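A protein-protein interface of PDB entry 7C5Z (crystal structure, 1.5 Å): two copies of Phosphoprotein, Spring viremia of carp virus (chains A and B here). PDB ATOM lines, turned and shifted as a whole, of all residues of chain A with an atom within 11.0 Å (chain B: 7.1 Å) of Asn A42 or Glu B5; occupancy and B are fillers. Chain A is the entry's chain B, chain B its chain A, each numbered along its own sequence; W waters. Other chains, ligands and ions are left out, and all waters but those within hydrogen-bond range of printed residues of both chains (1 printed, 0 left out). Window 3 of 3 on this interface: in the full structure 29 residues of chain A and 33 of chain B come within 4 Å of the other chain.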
ATOM      1  N   ILE A   9      21.803 -10.565   7.155  1.00  0.00           N
ATOM      2  CA  ILE A   9      21.195  -9.616   6.231  1.00  0.00           C
ATOM      3  C   ILE A   9      20.195 -10.314   5.324  1.00  0.00           C
ATOM      4  O   ILE A   9      20.408 -11.450   4.875  1.00  0.00           O
ATOM      5  CB  ILE A   9      22.292  -8.905   5.421  1.00  0.00           C
ATOM      6  CG1 ILE A   9      22.969  -7.832   6.281  1.00  0.00           C
ATOM      7  CG2 ILE A   9      21.719  -8.278   4.151  1.00  0.00           C
ATOM      8  CD1 ILE A   9      24.247  -7.329   5.688  1.00  0.00           C
ATOM      9  N   LEU A  36      20.772  -6.263  -4.117  1.00  0.00           N
ATOM     10  CA  LEU A  36      21.781  -5.396  -3.524  1.00  0.00           C
ATOM     11  C   LEU A  36      21.298  -3.960  -3.382  1.00  0.00           C
ATOM     12  O   LEU A  36      22.076  -3.099  -2.962  1.00  0.00           O
ATOM     13  CB  LEU A  36      23.069  -5.453  -4.351  1.00  0.00           C
ATOM     14  CG  LEU A  36      23.622  -6.880  -4.474  1.00  0.00           C
ATOM     15  CD1 LEU A  36      24.930  -6.916  -5.261  1.00  0.00           C
ATOM     16  CD2 LEU A  36      23.806  -7.489  -3.096  1.00  0.00           C
ATOM     17  N   GLY A  37      20.027  -3.695  -3.698  1.00  0.00           N
ATOM     18  CA  GLY A  37      19.530  -2.326  -3.674  1.00  0.00           C
ATOM     19  C   GLY A  37      19.575  -1.688  -2.297  1.00  0.00           C
ATOM     20  O   GLY A  37      19.885  -0.502  -2.165  1.00  0.00           O
ATOM     21  N   ASN A  38      19.261  -2.457  -1.253  1.00  0.00           N
ATOM     22  CA  ASN A  38      19.224  -1.924   0.104  1.00  0.00           C
ATOM     23  C   ASN A  38      20.517  -2.183   0.873  1.00  0.00           C
ATOM     24  O   ASN A  38      20.506  -2.204   2.108  1.00  0.00           O
ATOM     25  CB  ASN A  38      18.028  -2.487   0.870  1.00  0.00           C
ATOM     26  CG  ASN A  38      16.769  -1.660   0.671  1.00  0.00           C
ATOM     27  OD1 ASN A  38      15.773  -2.145   0.139  1.00  0.00           O
ATOM     28  ND2 ASN A  38      16.815  -0.398   1.093  1.00  0.00           N
ATOM     29  N   VAL A  39      21.621  -2.381   0.172  1.00  0.00           N
ATOM     30  CA  VAL A  39      22.939  -2.468   0.787  1.00  0.00           C
ATOM     31  C   VAL A  39      23.492  -1.058   0.968  1.00  0.00           C
ATOM     32  O   VAL A  39      23.351  -0.202   0.089  1.00  0.00           O
ATOM     33  CB  VAL A  39      23.869  -3.350  -0.073  1.00  0.00           C
ATOM     34  CG1 VAL A  39      25.324  -3.216   0.361  1.00  0.00           C
ATOM     35  CG2 VAL A  39      23.420  -4.804   0.010  1.00  0.00           C
ATOM     36  N   ASP A  40      24.078  -0.802   2.145  1.00  0.00           N
ATOM     37  CA  ASP A  40      24.825   0.405   2.495  1.00  0.00           C
ATOM     38  C   ASP A  40      25.761   0.815   1.360  1.00  0.00           C
ATOM     39  O   ASP A  40      26.499  -0.031   0.854  1.00  0.00           O
ATOM     40  CB  ASP A  40      25.603   0.111   3.784  1.00  0.00           C
ATOM     41  CG  ASP A  40      26.415   1.279   4.280  1.00  0.00           C
ATOM     42  OD1 ASP A  40      27.293   1.797   3.552  1.00  0.00           O
ATOM     43  OD2 ASP A  40      26.201   1.662   5.435  1.00  0.00           O
ATOM     44  N   PRO A  41      25.778   2.086   0.933  1.00  0.00           N
ATOM     45  CA  PRO A  41      26.658   2.456  -0.197  1.00  0.00           C
ATOM     46  C   PRO A  41      28.137   2.128   0.005  1.00  0.00           C
ATOM     47  O   PRO A  41      28.795   1.673  -0.943  1.00  0.00           O
ATOM     48  CB  PRO A  41      26.422   3.967  -0.331  1.00  0.00           C
ATOM     49  CG  PRO A  41      25.028   4.165   0.179  1.00  0.00           C
ATOM     50  CD  PRO A  41      24.895   3.199   1.329  1.00  0.00           C
ATOM     51  N   ASN A  42      28.689   2.338   1.206  1.00  0.00           N
ATOM     52  CA  ASN A  42      30.094   2.005   1.426  1.00  0.00           C
ATOM     53  C   ASN A  42      30.325   0.507   1.278  1.00  0.00           C
ATOM     54  O   ASN A  42      31.379   0.073   0.791  1.00  0.00           O
ATOM     55  CB  ASN A  42      30.549   2.474   2.810  1.00  0.00           C
ATOM     56  CG  ASN A  42      30.731   3.966   2.875  1.00  0.00           C
ATOM     57  OD1 ASN A  42      31.221   4.576   1.930  1.00  0.00           O
ATOM     58  ND2 ASN A  42      30.325   4.567   3.987  1.00  0.00           N
ATOM     59  N   TYR A  43      29.352  -0.303   1.692  1.00  0.00           N
ATOM     60  CA  TYR A  43      29.540  -1.742   1.618  1.00  0.00           C
ATOM     61  C   TYR A  43      29.181  -2.287   0.250  1.00  0.00           C
ATOM     62  O   TYR A  43      29.724  -3.326  -0.143  1.00  0.00           O
ATOM     63  CB  TYR A  43      28.757  -2.426   2.739  1.00  0.00           C
ATOM     64  CG  TYR A  43      29.497  -2.286   4.043  1.00  0.00           C
ATOM     65  CD1 TYR A  43      30.437  -3.229   4.440  1.00  0.00           C
ATOM     66  CD2 TYR A  43      29.304  -1.171   4.848  1.00  0.00           C
ATOM     67  CE1 TYR A  43      31.142  -3.085   5.638  1.00  0.00           C
ATOM     68  CE2 TYR A  43      29.998  -1.015   6.032  1.00  0.00           C
ATOM     69  CZ  TYR A  43      30.914  -1.967   6.422  1.00  0.00           C
ATOM     70  OH  TYR A  43      31.591  -1.804   7.604  1.00  0.00           O
ATOM     71  N   LYS A  44      28.314  -1.603  -0.506  1.00  0.00           N
ATOM     72  CA  LYS A  44      28.157  -1.986  -1.909  1.00  0.00           C
ATOM     73  C   LYS A  44      29.486  -1.866  -2.638  1.00  0.00           C
ATOM     74  O   LYS A  44      29.858  -2.753  -3.421  1.00  0.00           O
ATOM     75  CB  LYS A  44      27.085  -1.130  -2.597  1.00  0.00           C
ATOM     76  CG  LYS A  44      26.456  -1.812  -3.808  1.00  0.00           C
ATOM     77  CD  LYS A  44      25.355  -0.969  -4.439  1.00  0.00           C
ATOM     78  CE  LYS A  44      24.205  -0.731  -3.471  1.00  0.00           C
ATOM     79  NZ  LYS A  44      23.048  -0.064  -4.135  1.00  0.00           N
ATOM     80  N   ASN A  45      30.244  -0.805  -2.349  1.00  0.00           N
ATOM     81  CA  ASN A  45      31.564  -0.654  -2.955  1.00  0.00           C
ATOM     82  C   ASN A  45      32.507  -1.766  -2.498  1.00  0.00           C
ATOM     83  O   ASN A  45      33.200  -2.382  -3.317  1.00  0.00           O
ATOM     84  CB  ASN A  45      32.148   0.719  -2.619  1.00  0.00           C
ATOM     85  CG  ASN A  45      33.485   0.959  -3.293  1.00  0.00           C
ATOM     86  OD1 ASN A  45      33.568   1.042  -4.519  1.00  0.00           O
ATOM     87  ND2 ASN A  45      34.541   1.064  -2.494  1.00  0.00           N
ATOM     88  N   LEU A  46      32.531  -2.057  -1.196  1.00  0.00           N
ATOM     89  CA  LEU A  46      33.398  -3.122  -0.693  1.00  0.00           C
ATOM     90  C   LEU A  46      33.045  -4.472  -1.307  1.00  0.00           C
ATOM     91  O   LEU A  46      33.941  -5.246  -1.665  1.00  0.00           O
ATOM     92  CB  LEU A  46      33.314  -3.199   0.833  1.00  0.00           C
ATOM     93  CG  LEU A  46      34.170  -4.285   1.504  1.00  0.00           C
ATOM     94  CD1 LEU A  46      35.644  -4.049   1.227  1.00  0.00           C
ATOM     95  CD2 LEU A  46      33.911  -4.367   3.019  1.00  0.00           C
ATOM     96  N   ILE A  47      31.748  -4.788  -1.417  1.00  0.00           N
ATOM     97  CA  ILE A  47      31.357  -6.066  -2.012  1.00  0.00           C
ATOM     98  C   ILE A  47      31.879  -6.163  -3.437  1.00  0.00           C
ATOM     99  O   ILE A  47      32.429  -7.193  -3.853  1.00  0.00           O
ATOM    100  CB  ILE A  47      29.831  -6.232  -1.967  1.00  0.00           C
ATOM    101  CG1 ILE A  47      29.364  -6.502  -0.536  1.00  0.00           C
ATOM    102  CG2 ILE A  47      29.388  -7.357  -2.910  1.00  0.00           C
ATOM    103  CD1 ILE A  47      27.885  -6.247  -0.318  1.00  0.00           C
ATOM    104  N   SER A  48      31.709  -5.091  -4.208  1.00  0.00           N
ATOM    105  CA  SER A  48      32.138  -5.105  -5.605  1.00  0.00           C
ATOM    106  C   SER A  48      33.652  -5.254  -5.717  1.00  0.00           C
ATOM    107  O   SER A  48      34.148  -6.057  -6.523  1.00  0.00           O
ATOM    108  CB  SER A  48      31.656  -3.830  -6.303  1.00  0.00           C
ATOM    109  OG  SER A  48      31.924  -3.874  -7.694  1.00  0.00           O
ATOM    110  N   LYS A  49      34.406  -4.524  -4.888  1.00  0.00           N
ATOM    111  CA  LYS A  49      35.865  -4.590  -4.945  1.00  0.00           C
ATOM    112  C   LYS A  49      36.391  -5.950  -4.497  1.00  0.00           C
ATOM    113  O   LYS A  49      37.387  -6.452  -5.040  1.00  0.00           O
ATOM    114  CB  LYS A  49      36.466  -3.479  -4.084  1.00  0.00           C
ATOM    115  CG  LYS A  49      36.180  -2.083  -4.587  1.00  0.00           C
ATOM    116  CD  LYS A  49      36.921  -1.802  -5.879  1.00  0.00           C
ATOM    117  CE  LYS A  49      36.697  -0.364  -6.331  1.00  0.00           C
ATOM    118  NZ  LYS A  49      37.432   0.598  -5.464  1.00  0.00           N
ATOM    119  N   MET A  50      35.760  -6.553  -3.496  1.00  0.00           N
ATOM    120  CA  MET A  50      36.156  -7.875  -3.047  1.00  0.00           C
ATOM    121  C   MET A  50      35.902  -8.915  -4.124  1.00  0.00           C
ATOM    122  O   MET A  50      36.781  -9.738  -4.410  1.00  0.00           O
ATOM    123  CB  MET A  50      35.396  -8.256  -1.774  1.00  0.00           C
ATOM    124  CG  MET A  50      35.919  -7.654  -0.482  1.00  0.00           C
ATOM    125  SD  MET A  50      37.485  -8.566   0.250  1.00  0.00           S
ATOM    126  CE  MET A  50      37.401 -10.244  -0.757  1.00  0.00           C
ATOM    127  N   ASP A  70      29.186  -4.410 -12.856  1.00  0.00           N
ATOM    128  CA  ASP A  70      28.620  -3.663 -11.739  1.00  0.00           C
ATOM    129  C   ASP A  70      28.180  -2.330 -12.331  1.00  0.00           C
ATOM    130  O   ASP A  70      28.984  -1.406 -12.469  1.00  0.00           O
ATOM    131  CB  ASP A  70      29.649  -3.484 -10.624  1.00  0.00           C
ATOM    132  CG  ASP A  70      29.162  -2.569  -9.514  1.00  0.00           C
ATOM    133  OD1 ASP A  70      27.952  -2.253  -9.472  1.00  0.00           O
ATOM    134  OD2 ASP A  70      30.001  -2.162  -8.681  1.00  0.00           O
ATOM    135  N   LEU A  76      24.949  -7.559  -9.161  1.00  0.00           N
ATOM    136  CA  LEU A  76      26.259  -7.795  -9.747  1.00  0.00           C
ATOM    137  C   LEU A  76      26.175  -9.052 -10.592  1.00  0.00           C
ATOM    138  O   LEU A  76      25.432  -9.985 -10.261  1.00  0.00           O
ATOM    139  CB  LEU A  76      27.354  -7.996  -8.681  1.00  0.00           C
ATOM    140  CG  LEU A  76      27.694  -6.901  -7.675  1.00  0.00           C
ATOM    141  CD1 LEU A  76      28.567  -7.491  -6.582  1.00  0.00           C
ATOM    142  CD2 LEU A  76      28.405  -5.763  -8.363  1.00  0.00           C
ATOM    143  N   TRP B   2      18.535  12.686   3.402  1.00  0.00           N
ATOM    144  CA  TRP B   2      19.791  12.500   4.114  1.00  0.00           C
ATOM    145  C   TRP B   2      20.655  11.477   3.391  1.00  0.00           C
ATOM    146  O   TRP B   2      20.149  10.489   2.850  1.00  0.00           O
ATOM    147  CB  TRP B   2      19.547  12.051   5.560  1.00  0.00           C
ATOM    148  CG  TRP B   2      20.802  11.703   6.303  1.00  0.00           C
ATOM    149  CD1 TRP B   2      21.295  10.450   6.541  1.00  0.00           C
ATOM    150  CD2 TRP B   2      21.729  12.618   6.902  1.00  0.00           C
ATOM    151  NE1 TRP B   2      22.467  10.529   7.258  1.00  0.00           N
ATOM    152  CE2 TRP B   2      22.758  11.848   7.487  1.00  0.00           C
ATOM    153  CE3 TRP B   2      21.789  14.012   7.004  1.00  0.00           C
ATOM    154  CZ2 TRP B   2      23.833  12.427   8.162  1.00  0.00           C
ATOM    155  CZ3 TRP B   2      22.859  14.583   7.674  1.00  0.00           C
ATOM    156  CH2 TRP B   2      23.866  13.791   8.245  1.00  0.00           C
ATOM    157  N   GLU B   3      21.963  11.719   3.396  1.00  0.00           N
ATOM    158  CA  GLU B   3      22.923  10.843   2.737  1.00  0.00           C
ATOM    159  C   GLU B   3      24.262  10.973   3.449  1.00  0.00           C
ATOM    160  O   GLU B   3      24.708  12.089   3.732  1.00  0.00           O
ATOM    161  CB  GLU B   3      23.058  11.195   1.250  1.00  0.00           C
ATOM    162  CG  GLU B   3      24.026  10.324   0.477  1.00  0.00           C
ATOM    163  CD  GLU B   3      24.584  11.027  -0.745  1.00  0.00           C
ATOM    164  OE1 GLU B   3      23.961  12.011  -1.201  1.00  0.00           O
ATOM    165  OE2 GLU B   3      25.641  10.594  -1.253  1.00  0.00           O
ATOM    166  N   GLU B   4      24.888   9.839   3.749  1.00  0.00           N
ATOM    167  CA  GLU B   4      26.161   9.838   4.454  1.00  0.00           C
ATOM    168  C   GLU B   4      27.335   9.909   3.475  1.00  0.00           C
ATOM    169  O   GLU B   4      27.183   9.773   2.262  1.00  0.00           O
ATOM    170  CB  GLU B   4      26.287   8.596   5.338  1.00  0.00           C
ATOM    171  CG  GLU B   4      25.070   8.293   6.194  1.00  0.00           C
ATOM    172  CD  GLU B   4      25.187   8.827   7.611  1.00  0.00           C
ATOM    173  OE1 GLU B   4      24.209   8.690   8.381  1.00  0.00           O
ATOM    174  OE2 GLU B   4      26.257   9.374   7.955  1.00  0.00           O
ATOM    175  N   GLU B   5      28.521  10.134   4.029  1.00  0.00           N
ATOM    176  CA  GLU B   5      29.754  10.134   3.258  1.00  0.00           C
ATOM    177  C   GLU B   5      30.007   8.740   2.696  1.00  0.00           C
ATOM    178  O   GLU B   5      29.938   7.746   3.422  1.00  0.00           O
ATOM    179  CB  GLU B   5      30.915  10.559   4.156  1.00  0.00           C
ATOM    180  CG  GLU B   5      31.122  12.053   4.290  1.00  0.00           C
ATOM    181  CD  GLU B   5      32.284  12.375   5.210  1.00  0.00           C
ATOM    182  OE1 GLU B   5      33.017  11.428   5.569  1.00  0.00           O
ATOM    183  OE2 GLU B   5      32.456  13.557   5.585  1.00  0.00           O
ATOM    184  N   SER B   6      30.318   8.662   1.409  1.00  0.00           N
ATOM    185  CA  SER B   6      30.700   7.390   0.794  1.00  0.00           C
ATOM    186  C   SER B   6      32.066   7.570   0.143  1.00  0.00           C
ATOM    187  O   SER B   6      32.182   7.692  -1.080  1.00  0.00           O
ATOM    188  CB  SER B   6      29.636   6.874  -0.232  1.00  0.00           C
ATOM    189  OG  SER B   6      29.449   7.771  -1.297  1.00  0.00           O
ATOM    190  N   THR B   7      33.106   7.592   0.978  1.00  0.00           N
ATOM    191  CA  THR B   7      34.481   7.744   0.519  1.00  0.00           C
ATOM    192  C   THR B   7      35.199   6.416   0.322  1.00  0.00           C
ATOM    193  O   THR B   7      36.019   6.301  -0.595  1.00  0.00           O
ATOM    194  CB  THR B   7      35.284   8.602   1.506  1.00  0.00           C
ATOM    195  OG1 THR B   7      34.872   8.309   2.846  1.00  0.00           O
ATOM    196  CG2 THR B   7      35.070  10.084   1.229  1.00  0.00           C
ATOM    197  N   GLY B   8      34.922   5.418   1.160  1.00  0.00           N
ATOM    198  CA  GLY B   8      35.530   4.111   0.999  1.00  0.00           C
ATOM    199  C   GLY B   8      36.091   3.512   2.275  1.00  0.00           C
ATOM    200  O   GLY B   8      36.822   4.177   3.017  1.00  0.00           O
ATOM    201  N   ILE B   9      35.759   2.246   2.535  1.00  0.00           N
ATOM    202  CA  ILE B   9      36.284   1.547   3.702  1.00  0.00           C
ATOM    203  C   ILE B   9      37.768   1.269   3.501  1.00  0.00           C
ATOM    204  O   ILE B   9      38.190   0.795   2.437  1.00  0.00           O
ATOM    205  CB  ILE B   9      35.502   0.247   3.937  1.00  0.00           C
ATOM    206  CG1 ILE B   9      34.060   0.561   4.342  1.00  0.00           C
ATOM    207  CG2 ILE B   9      36.175  -0.605   4.995  1.00  0.00           C
ATOM    208  CD1 ILE B   9      33.113  -0.542   4.016  1.00  0.00           C
HETATM  209  O   HOH W   1      34.217   0.833   0.440  1.00  0.00           O
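Printed residues of chain B within 4 Å of Asn A42: Glu B5 (3.3 Å), Ser B6 (3.1 Å), Thr B7 (3.7 Å), Gly B8 (3.9 Å) and Ile B9 (3.7 Å).
Printed residues of chain B within 4 Å of Tyr A43: Ile B9.
Leu A46 touches none of the printed residues of chain B.
Asp A70 touches none of the printed residues of chain B.
No residue of chain A comes within 4 Å of Glu B4.
Of chain A, only Asn A42 (3.3 Å) comes within 4 Å of Glu B5.
Of chain A, only Asn A42 (3.1 Å) comes within 4 Å of Ser B6.
Thr B7 touches just one residue of chain A: Asn A42 (3.7 Å).
Gly B8 touches just one residue of chain A: Asn A42.
Printed residues of chain A within 4 Å of Ile B9: Asn A42 (3.7 Å) and Tyr A43 (3.6 Å).
The nearest residue of chain A that does not touch Glu B5 is Pro A41 (6.4 Å).
Water W1 lies within hydrogen-bond range of the backbone carbonyl oxygen (O) of Asn A42 (3.0 Å), the backbone NH (N) of Ile B9 (3.0 Å) and the side-chain amide nitrogen (ND2) of Asn A45 (3.0 Å).
Among the printed residues, pairs that only touch across the chains: Asn A42 with Ser B6 (3.1 Å), Asn A42 with Thr B7 (3.7 Å), Asn A42 with Gly B8 (3.9 Å), Asn A42 with Ile B9 (3.7 Å) and Tyr A43 with Ile B9 (3.6 Å).
Printed residues of chain B that touch a printed residue of chain A: Glu B5, Ser B6, Thr B7, Gly B8 and Ile B9.
Hydrophobic or aromatic side chains of chain B within 4 Å of the printed part of chain A: Ile B9.
Along chain B the printed residues that touch a printed residue of chain A span positions 5 to 9.
The backbone carbonyl oxygen (O) of Glu B5 lies within hydrogen-bond range of the side-chain amide nitrogen (ND2) of Asn A42 (3.3 Å).
OD1 of Asp A40 sits at hydrogen-bond distance from N of Asn A42, at 2.8 Å.
N of Tyr A43 lies within hydrogen-bond range of OD1 of Asp A40, 3.5 Å away.
Position printed for both chains: 9.
Of the 6 pairs that touch across the chains among the printed residues, none has its exchanged pair printed and touching as well.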
